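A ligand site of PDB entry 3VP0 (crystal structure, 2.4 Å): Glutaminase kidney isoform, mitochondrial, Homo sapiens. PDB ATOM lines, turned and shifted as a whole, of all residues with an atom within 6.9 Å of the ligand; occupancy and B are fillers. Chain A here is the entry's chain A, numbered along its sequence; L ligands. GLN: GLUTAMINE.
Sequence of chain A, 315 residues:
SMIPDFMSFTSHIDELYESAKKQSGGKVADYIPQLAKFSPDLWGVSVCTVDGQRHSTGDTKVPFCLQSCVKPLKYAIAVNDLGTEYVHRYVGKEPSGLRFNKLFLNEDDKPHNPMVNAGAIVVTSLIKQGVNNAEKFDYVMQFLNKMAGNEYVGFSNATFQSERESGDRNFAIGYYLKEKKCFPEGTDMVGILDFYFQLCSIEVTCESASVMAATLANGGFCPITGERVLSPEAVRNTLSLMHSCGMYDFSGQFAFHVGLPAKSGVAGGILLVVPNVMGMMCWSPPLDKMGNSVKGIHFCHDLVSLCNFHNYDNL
OH of Tyr 196 is in hydrogen-bond range of OXT of the ligand, 2.7 Å away. NE2 of the ligand sits close to OG of Ser 68 (2.8 Å). An oxygen (OE1) of the ligand is in hydrogen-bond range of the side-chain hydroxyl of Tyr 248 (2.8 Å). The side-chain amide nitrogen of Asn 117 lies within hydrogen-bond range of an oxygen (O) of the ligand (2.9 Å). The side-chain carboxylate (OE2) of Glu 163 is in salt-bridge range of a nitrogen (N) of the ligand. OE1 of Gln 67 is in hydrogen-bond range of N of the ligand. ND2 of Asn 170 lies within hydrogen-bond range of O of the ligand, at 3.3 Å. The side-chain hydroxyl (OH) of Tyr 31 sits close to a nitrogen (N) of the ligand, at 3.5 Å.
The side-chain hydroxyl (OH) of Tyr 196 is in hydrogen-bond range of the side-chain amino group (NZ) of Lys 71 (3.0 Å). OG of Ser 68 is in hydrogen-bond range of NZ of Lys 71 (3.0 Å). The backbone NH (N) of Val 266 sits at hydrogen-bond distance from the side-chain hydroxyl (OH) of Tyr 248 (3.5 Å). The side-chain amide nitrogen (ND2) of Asn 117 sits at hydrogen-bond distance from the side-chain amide oxygen (OD1) of Asn 170, 2.8 Å away. The side-chain amide oxygen (OD1) of Asn 117 lies within hydrogen-bond range of the side-chain amino group (NZ) of Lys 71, at 3.5 Å. The side-chain carboxylate (OE1) of Glu 163 is in hydrogen-bond range of the side-chain hydroxyl (OH) of Tyr 31, at 2.5 Å. The backbone NH (N) of Gln 67 is in hydrogen-bond range of the backbone carbonyl oxygen (O) of Cys 200, at 3.1 Å. N of Gly 265 sits at hydrogen-bond distance from SG of Cys 69 (3.5 Å).
The backbone NH of Val 266 sits close to a nitrogen (NE2) of the ligand (3.0 Å). Cys 200 touches the ligand (SG to N, 3.9 Å). CA of Gly 265 touches NE2 of the ligand (3.6 Å). Hydrophobic or aromatic side chains that line the ligand: Tyr 196, Tyr 248 and Val 266. Of the 23 residues printed, 11 come within 4 Å of the ligand.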
ATOM      1  N   TYR A  31       3.869   1.911  21.228  1.00  0.00           N
ATOM      2  CA  TYR A  31       2.602   1.509  20.654  1.00  0.00           C
ATOM      3  C   TYR A  31       2.323   0.039  20.938  1.00  0.00           C
ATOM      4  O   TYR A  31       1.191  -0.428  20.801  1.00  0.00           O
ATOM      5  CB  TYR A  31       2.561   1.832  19.145  1.00  0.00           C
ATOM      6  CG  TYR A  31       3.501   1.052  18.296  1.00  0.00           C
ATOM      7  CD1 TYR A  31       3.135  -0.186  17.771  1.00  0.00           C
ATOM      8  CD2 TYR A  31       4.766   1.552  17.980  1.00  0.00           C
ATOM      9  CE1 TYR A  31       3.990  -0.898  16.949  1.00  0.00           C
ATOM     10  CE2 TYR A  31       5.633   0.841  17.171  1.00  0.00           C
ATOM     11  CZ  TYR A  31       5.238  -0.389  16.646  1.00  0.00           C
ATOM     12  OH  TYR A  31       6.092  -1.105  15.833  1.00  0.00           O
ATOM     13  N   ILE A  32       3.369  -0.690  21.330  1.00  0.00           N
ATOM     14  CA  ILE A  32       3.266  -2.099  21.737  1.00  0.00           C
ATOM     15  C   ILE A  32       4.183  -2.231  22.957  1.00  0.00           C
ATOM     16  O   ILE A  32       5.181  -1.516  23.069  1.00  0.00           O
ATOM     17  CB  ILE A  32       3.688  -3.124  20.657  1.00  0.00           C
ATOM     18  CG1 ILE A  32       5.081  -2.811  20.115  1.00  0.00           C
ATOM     19  CG2 ILE A  32       2.651  -3.154  19.549  1.00  0.00           C
ATOM     20  CD1 ILE A  32       5.625  -3.909  19.200  1.00  0.00           C
ATOM     21  N   LEU A  35       8.152  -2.745  22.879  1.00  0.00           N
ATOM     22  CA  LEU A  35       9.027  -1.612  22.627  1.00  0.00           C
ATOM     23  C   LEU A  35       9.103  -0.725  23.861  1.00  0.00           C
ATOM     24  O   LEU A  35      10.186  -0.197  24.179  1.00  0.00           O
ATOM     25  CB  LEU A  35       8.526  -0.802  21.417  1.00  0.00           C
ATOM     26  CG  LEU A  35       8.792  -1.469  20.064  1.00  0.00           C
ATOM     27  CD1 LEU A  35       7.983  -0.786  18.977  1.00  0.00           C
ATOM     28  CD2 LEU A  35      10.297  -1.438  19.762  1.00  0.00           C
ATOM     29  N   LEU A  66      14.878  -5.370  14.357  1.00  0.00           N
ATOM     30  CA  LEU A  66      15.277  -4.531  13.227  1.00  0.00           C
ATOM     31  C   LEU A  66      14.183  -3.521  12.901  1.00  0.00           C
ATOM     32  O   LEU A  66      14.476  -2.332  12.727  1.00  0.00           O
ATOM     33  CB  LEU A  66      15.538  -5.395  11.989  1.00  0.00           C
ATOM     34  CG  LEU A  66      16.946  -5.999  11.848  1.00  0.00           C
ATOM     35  CD1 LEU A  66      16.943  -7.066  10.768  1.00  0.00           C
ATOM     36  CD2 LEU A  66      17.957  -4.892  11.528  1.00  0.00           C
ATOM     37  N   GLN A  67      12.943  -3.984  12.859  1.00  0.00           N
ATOM     38  CA  GLN A  67      11.807  -3.129  12.520  1.00  0.00           C
ATOM     39  C   GLN A  67      12.062  -2.564  11.122  1.00  0.00           C
ATOM     40  O   GLN A  67      12.381  -3.335  10.213  1.00  0.00           O
ATOM     41  CB  GLN A  67      11.648  -2.002  13.550  1.00  0.00           C
ATOM     42  CG  GLN A  67      11.069  -2.455  14.886  1.00  0.00           C
ATOM     43  CD  GLN A  67       9.692  -3.113  14.759  1.00  0.00           C
ATOM     44  OE1 GLN A  67       9.138  -3.195  13.666  1.00  0.00           O
ATOM     45  NE2 GLN A  67       9.141  -3.579  15.879  1.00  0.00           N
ATOM     46  N   SER A  68      11.950  -1.260  10.924  1.00  0.00           N
ATOM     47  CA  SER A  68      12.167  -0.730   9.594  1.00  0.00           C
ATOM     48  C   SER A  68      13.593  -0.892   9.079  1.00  0.00           C
ATOM     49  O   SER A  68      13.850  -0.743   7.879  1.00  0.00           O
ATOM     50  CB  SER A  68      11.753   0.746   9.521  1.00  0.00           C
ATOM     51  OG  SER A  68      10.330   0.825   9.382  1.00  0.00           O
ATOM     52  N   CYS A  69      14.527  -1.220   9.970  1.00  0.00           N
ATOM     53  CA  CYS A  69      15.903  -1.387   9.538  1.00  0.00           C
ATOM     54  C   CYS A  69      16.049  -2.576   8.589  1.00  0.00           C
ATOM     55  O   CYS A  69      17.027  -2.677   7.864  1.00  0.00           O
ATOM     56  CB  CYS A  69      16.826  -1.572  10.744  1.00  0.00           C
ATOM     57  SG  CYS A  69      16.966  -0.088  11.750  1.00  0.00           S
ATOM     58  N   LYS A  71      13.927  -3.174   6.115  1.00  0.00           N
ATOM     59  CA  LYS A  71      13.429  -2.772   4.795  1.00  0.00           C
ATOM     60  C   LYS A  71      14.507  -2.748   3.704  1.00  0.00           C
ATOM     61  O   LYS A  71      14.351  -3.373   2.659  1.00  0.00           O
ATOM     62  CB  LYS A  71      12.722  -1.413   4.885  1.00  0.00           C
ATOM     63  CG  LYS A  71      11.344  -1.489   5.545  1.00  0.00           C
ATOM     64  CD  LYS A  71      10.733  -0.091   5.685  1.00  0.00           C
ATOM     65  CE  LYS A  71       9.243  -0.144   6.022  1.00  0.00           C
ATOM     66  NZ  LYS A  71       8.993  -0.836   7.326  1.00  0.00           N
ATOM     67  N   ASN A 117       6.288   1.915   4.364  1.00  0.00           N
ATOM     68  CA  ASN A 117       5.533   0.689   4.615  1.00  0.00           C
ATOM     69  C   ASN A 117       4.911   0.047   3.387  1.00  0.00           C
ATOM     70  O   ASN A 117       5.169  -1.136   3.110  1.00  0.00           O
ATOM     71  CB  ASN A 117       4.465   0.945   5.675  1.00  0.00           C
ATOM     72  CG  ASN A 117       5.044   1.036   7.076  1.00  0.00           C
ATOM     73  OD1 ASN A 117       6.244   1.282   7.266  1.00  0.00           O
ATOM     74  ND2 ASN A 117       4.191   0.856   8.076  1.00  0.00           N
ATOM     75  N   THR A 159       7.019  -9.636  19.811  1.00  0.00           N
ATOM     76  CA  THR A 159       6.923  -8.482  18.950  1.00  0.00           C
ATOM     77  C   THR A 159       6.008  -8.826  17.776  1.00  0.00           C
ATOM     78  O   THR A 159       5.043  -8.122  17.524  1.00  0.00           O
ATOM     79  CB  THR A 159       8.314  -8.062  18.426  1.00  0.00           C
ATOM     80  OG1 THR A 159       9.135  -7.629  19.524  1.00  0.00           O
ATOM     81  CG2 THR A 159       8.180  -6.913  17.436  1.00  0.00           C
ATOM     82  N   GLU A 163       2.715  -6.838  16.891  1.00  0.00           N
ATOM     83  CA  GLU A 163       2.735  -6.086  15.642  1.00  0.00           C
ATOM     84  C   GLU A 163       1.507  -6.416  14.816  1.00  0.00           C
ATOM     85  O   GLU A 163       0.807  -5.537  14.349  1.00  0.00           O
ATOM     86  CB  GLU A 163       4.009  -6.426  14.837  1.00  0.00           C
ATOM     87  CG  GLU A 163       5.270  -5.760  15.349  1.00  0.00           C
ATOM     88  CD  GLU A 163       5.320  -4.258  15.084  1.00  0.00           C
ATOM     89  OE1 GLU A 163       6.159  -3.564  15.708  1.00  0.00           O
ATOM     90  OE2 GLU A 163       4.534  -3.765  14.241  1.00  0.00           O
ATOM     91  N   ARG A 169      -3.215   0.013  10.633  1.00  0.00           N
ATOM     92  CA  ARG A 169      -2.780   0.829   9.506  1.00  0.00           C
ATOM     93  C   ARG A 169      -2.123  -0.004   8.418  1.00  0.00           C
ATOM     94  O   ARG A 169      -2.359   0.233   7.230  1.00  0.00           O
ATOM     95  CB  ARG A 169      -1.830   1.937   9.963  1.00  0.00           C
ATOM     96  CG  ARG A 169      -1.406   2.833   8.819  1.00  0.00           C
ATOM     97  CD  ARG A 169      -0.693   4.101   9.300  1.00  0.00           C
ATOM     98  NE  ARG A 169      -0.260   4.944   8.186  1.00  0.00           N
ATOM     99  CZ  ARG A 169       0.885   4.800   7.522  1.00  0.00           C
ATOM    100  NH1 ARG A 169       1.745   3.842   7.853  1.00  0.00           N
ATOM    101  NH2 ARG A 169       1.180   5.615   6.517  1.00  0.00           N
ATOM    102  N   ASN A 170      -1.308  -0.987   8.800  1.00  0.00           N
ATOM    103  CA  ASN A 170      -0.663  -1.839   7.802  1.00  0.00           C
ATOM    104  C   ASN A 170      -1.714  -2.705   7.110  1.00  0.00           C
ATOM    105  O   ASN A 170      -1.563  -3.045   5.929  1.00  0.00           O
ATOM    106  CB  ASN A 170       0.427  -2.717   8.415  1.00  0.00           C
ATOM    107  CG  ASN A 170       1.671  -1.936   8.804  1.00  0.00           C
ATOM    108  OD1 ASN A 170       2.189  -1.136   8.023  1.00  0.00           O
ATOM    109  ND2 ASN A 170       2.176  -2.178  10.013  1.00  0.00           N
ATOM    110  N   TYR A 196       5.439  -9.959   6.553  1.00  0.00           N
ATOM    111  CA  TYR A 196       5.939  -8.601   6.814  1.00  0.00           C
ATOM    112  C   TYR A 196       6.170  -8.354   8.306  1.00  0.00           C
ATOM    113  O   TYR A 196       7.224  -7.828   8.710  1.00  0.00           O
ATOM    114  CB  TYR A 196       4.944  -7.571   6.261  1.00  0.00           C
ATOM    115  CG  TYR A 196       5.304  -6.125   6.587  1.00  0.00           C
ATOM    116  CD1 TYR A 196       6.326  -5.470   5.901  1.00  0.00           C
ATOM    117  CD2 TYR A 196       4.646  -5.440   7.602  1.00  0.00           C
ATOM    118  CE1 TYR A 196       6.694  -4.155   6.230  1.00  0.00           C
ATOM    119  CE2 TYR A 196       4.992  -4.133   7.936  1.00  0.00           C
ATOM    120  CZ  TYR A 196       6.017  -3.502   7.250  1.00  0.00           C
ATOM    121  OH  TYR A 196       6.369  -2.211   7.589  1.00  0.00           O
ATOM    122  N   PHE A 197       5.181  -8.707   9.131  1.00  0.00           N
ATOM    123  CA  PHE A 197       5.285  -8.539  10.574  1.00  0.00           C
ATOM    124  C   PHE A 197       6.427  -9.366  11.149  1.00  0.00           C
ATOM    125  O   PHE A 197       7.141  -8.915  12.045  1.00  0.00           O
ATOM    126  CB  PHE A 197       3.958  -8.934  11.238  1.00  0.00           C
ATOM    127  CG  PHE A 197       2.831  -8.008  10.913  1.00  0.00           C
ATOM    128  CD1 PHE A 197       1.577  -8.514  10.557  1.00  0.00           C
ATOM    129  CD2 PHE A 197       3.007  -6.630  10.955  1.00  0.00           C
ATOM    130  CE1 PHE A 197       0.518  -7.651  10.252  1.00  0.00           C
ATOM    131  CE2 PHE A 197       1.959  -5.761  10.653  1.00  0.00           C
ATOM    132  CZ  PHE A 197       0.714  -6.274  10.306  1.00  0.00           C
ATOM    133  N   CYS A 200       9.778  -7.799  10.474  1.00  0.00           N
ATOM    134  CA  CYS A 200       9.961  -6.641  11.346  1.00  0.00           C
ATOM    135  C   CYS A 200      10.396  -7.100  12.722  1.00  0.00           C
ATOM    136  O   CYS A 200      10.991  -6.328  13.487  1.00  0.00           O
ATOM    137  CB  CYS A 200       8.651  -5.859  11.493  1.00  0.00           C
ATOM    138  SG  CYS A 200       8.167  -4.870  10.060  1.00  0.00           S
ATOM    139  N   TYR A 248      12.921   8.326   7.413  1.00  0.00           N
ATOM    140  CA  TYR A 248      11.551   8.846   7.517  1.00  0.00           C
ATOM    141  C   TYR A 248      11.570  10.276   6.956  1.00  0.00           C
ATOM    142  O   TYR A 248      12.275  10.555   5.981  1.00  0.00           O
ATOM    143  CB  TYR A 248      11.065   8.850   8.973  1.00  0.00           C
ATOM    144  CG  TYR A 248      11.122   7.493   9.665  1.00  0.00           C
ATOM    145  CD1 TYR A 248      10.391   6.397   9.177  1.00  0.00           C
ATOM    146  CD2 TYR A 248      11.895   7.296  10.819  1.00  0.00           C
ATOM    147  CE1 TYR A 248      10.426   5.161   9.826  1.00  0.00           C
ATOM    148  CE2 TYR A 248      11.932   6.069  11.472  1.00  0.00           C
ATOM    149  CZ  TYR A 248      11.198   5.001  10.975  1.00  0.00           C
ATOM    150  OH  TYR A 248      11.227   3.781  11.620  1.00  0.00           O
ATOM    151  N   LYS A 263      19.418   3.838   7.518  1.00  0.00           N
ATOM    152  CA  LYS A 263      18.052   3.410   7.705  1.00  0.00           C
ATOM    153  C   LYS A 263      17.767   3.310   9.183  1.00  0.00           C
ATOM    154  O   LYS A 263      18.443   2.573   9.908  1.00  0.00           O
ATOM    155  CB  LYS A 263      17.782   2.045   7.058  1.00  0.00           C
ATOM    156  CG  LYS A 263      16.313   1.638   7.123  1.00  0.00           C
ATOM    157  CD  LYS A 263      15.443   2.528   6.233  1.00  0.00           C
ATOM    158  CE  LYS A 263      13.947   2.416   6.530  1.00  0.00           C
ATOM    159  NZ  LYS A 263      13.498   3.379   7.588  1.00  0.00           N
ATOM    160  N   SER A 264      16.773   4.062   9.644  1.00  0.00           N
ATOM    161  CA  SER A 264      16.407   4.020  11.055  1.00  0.00           C
ATOM    162  C   SER A 264      15.201   3.093  11.268  1.00  0.00           C
ATOM    163  O   SER A 264      14.513   2.709  10.318  1.00  0.00           O
ATOM    164  CB  SER A 264      16.114   5.430  11.564  1.00  0.00           C
ATOM    165  OG  SER A 264      15.047   6.011  10.863  1.00  0.00           O
ATOM    166  N   GLY A 265      14.999   2.712  12.527  1.00  0.00           N
ATOM    167  CA  GLY A 265      13.896   1.832  12.906  1.00  0.00           C
ATOM    168  C   GLY A 265      13.279   2.354  14.192  1.00  0.00           C
ATOM    169  O   GLY A 265      13.928   3.094  14.945  1.00  0.00           O
ATOM    170  N   VAL A 266      12.029   1.961  14.450  1.00  0.00           N
ATOM    171  CA  VAL A 266      11.307   2.413  15.637  1.00  0.00           C
ATOM    172  C   VAL A 266      11.903   1.838  16.925  1.00  0.00           C
ATOM    173  O   VAL A 266      11.703   2.362  18.024  1.00  0.00           O
ATOM    174  CB  VAL A 266       9.786   2.038  15.512  1.00  0.00           C
ATOM    175  CG1 VAL A 266       9.606   0.528  15.684  1.00  0.00           C
ATOM    176  CG2 VAL A 266       8.959   2.831  16.499  1.00  0.00           C
ATOM    177  N   ALA A 267      12.669   0.750  16.793  1.00  0.00           N
ATOM    178  CA  ALA A 267      13.299   0.128  17.950  1.00  0.00           C
ATOM    179  C   ALA A 267      14.433   1.022  18.452  1.00  0.00           C
ATOM    180  O   ALA A 267      14.969   0.799  19.539  1.00  0.00           O
ATOM    181  CB  ALA A 267      13.844  -1.250  17.580  1.00  0.00           C
ATOM    182  N   GLY A 291      10.936  10.183  14.617  1.00  0.00           N
ATOM    183  CA  GLY A 291      10.977   8.736  14.750  1.00  0.00           C
ATOM    184  C   GLY A 291      12.387   8.159  14.712  1.00  0.00           C
ATOM    185  O   GLY A 291      12.561   6.944  14.612  1.00  0.00           O
HETATM  186  N   GLN L   1       6.522  -2.396  12.648  1.00  0.00           N
HETATM  187  CA  GLN L   1       5.959  -1.029  12.420  1.00  0.00           C
HETATM  188  C   GLN L   1       5.368  -0.927  11.012  1.00  0.00           C
HETATM  189  O   GLN L   1       4.554  -0.009  10.777  1.00  0.00           O
HETATM  190  CB  GLN L   1       7.045   0.047  12.615  1.00  0.00           C
HETATM  191  CG  GLN L   1       8.253  -0.051  11.689  1.00  0.00           C
HETATM  192  CD  GLN L   1       9.242   1.088  11.907  1.00  0.00           C
HETATM  193  OE1 GLN L   1       8.882   2.258  11.812  1.00  0.00           O
HETATM  194  NE2 GLN L   1      10.499   0.742  12.203  1.00  0.00           N
HETATM  195  OXT GLN L   1       5.733  -1.770  10.150  1.00  0.00           O
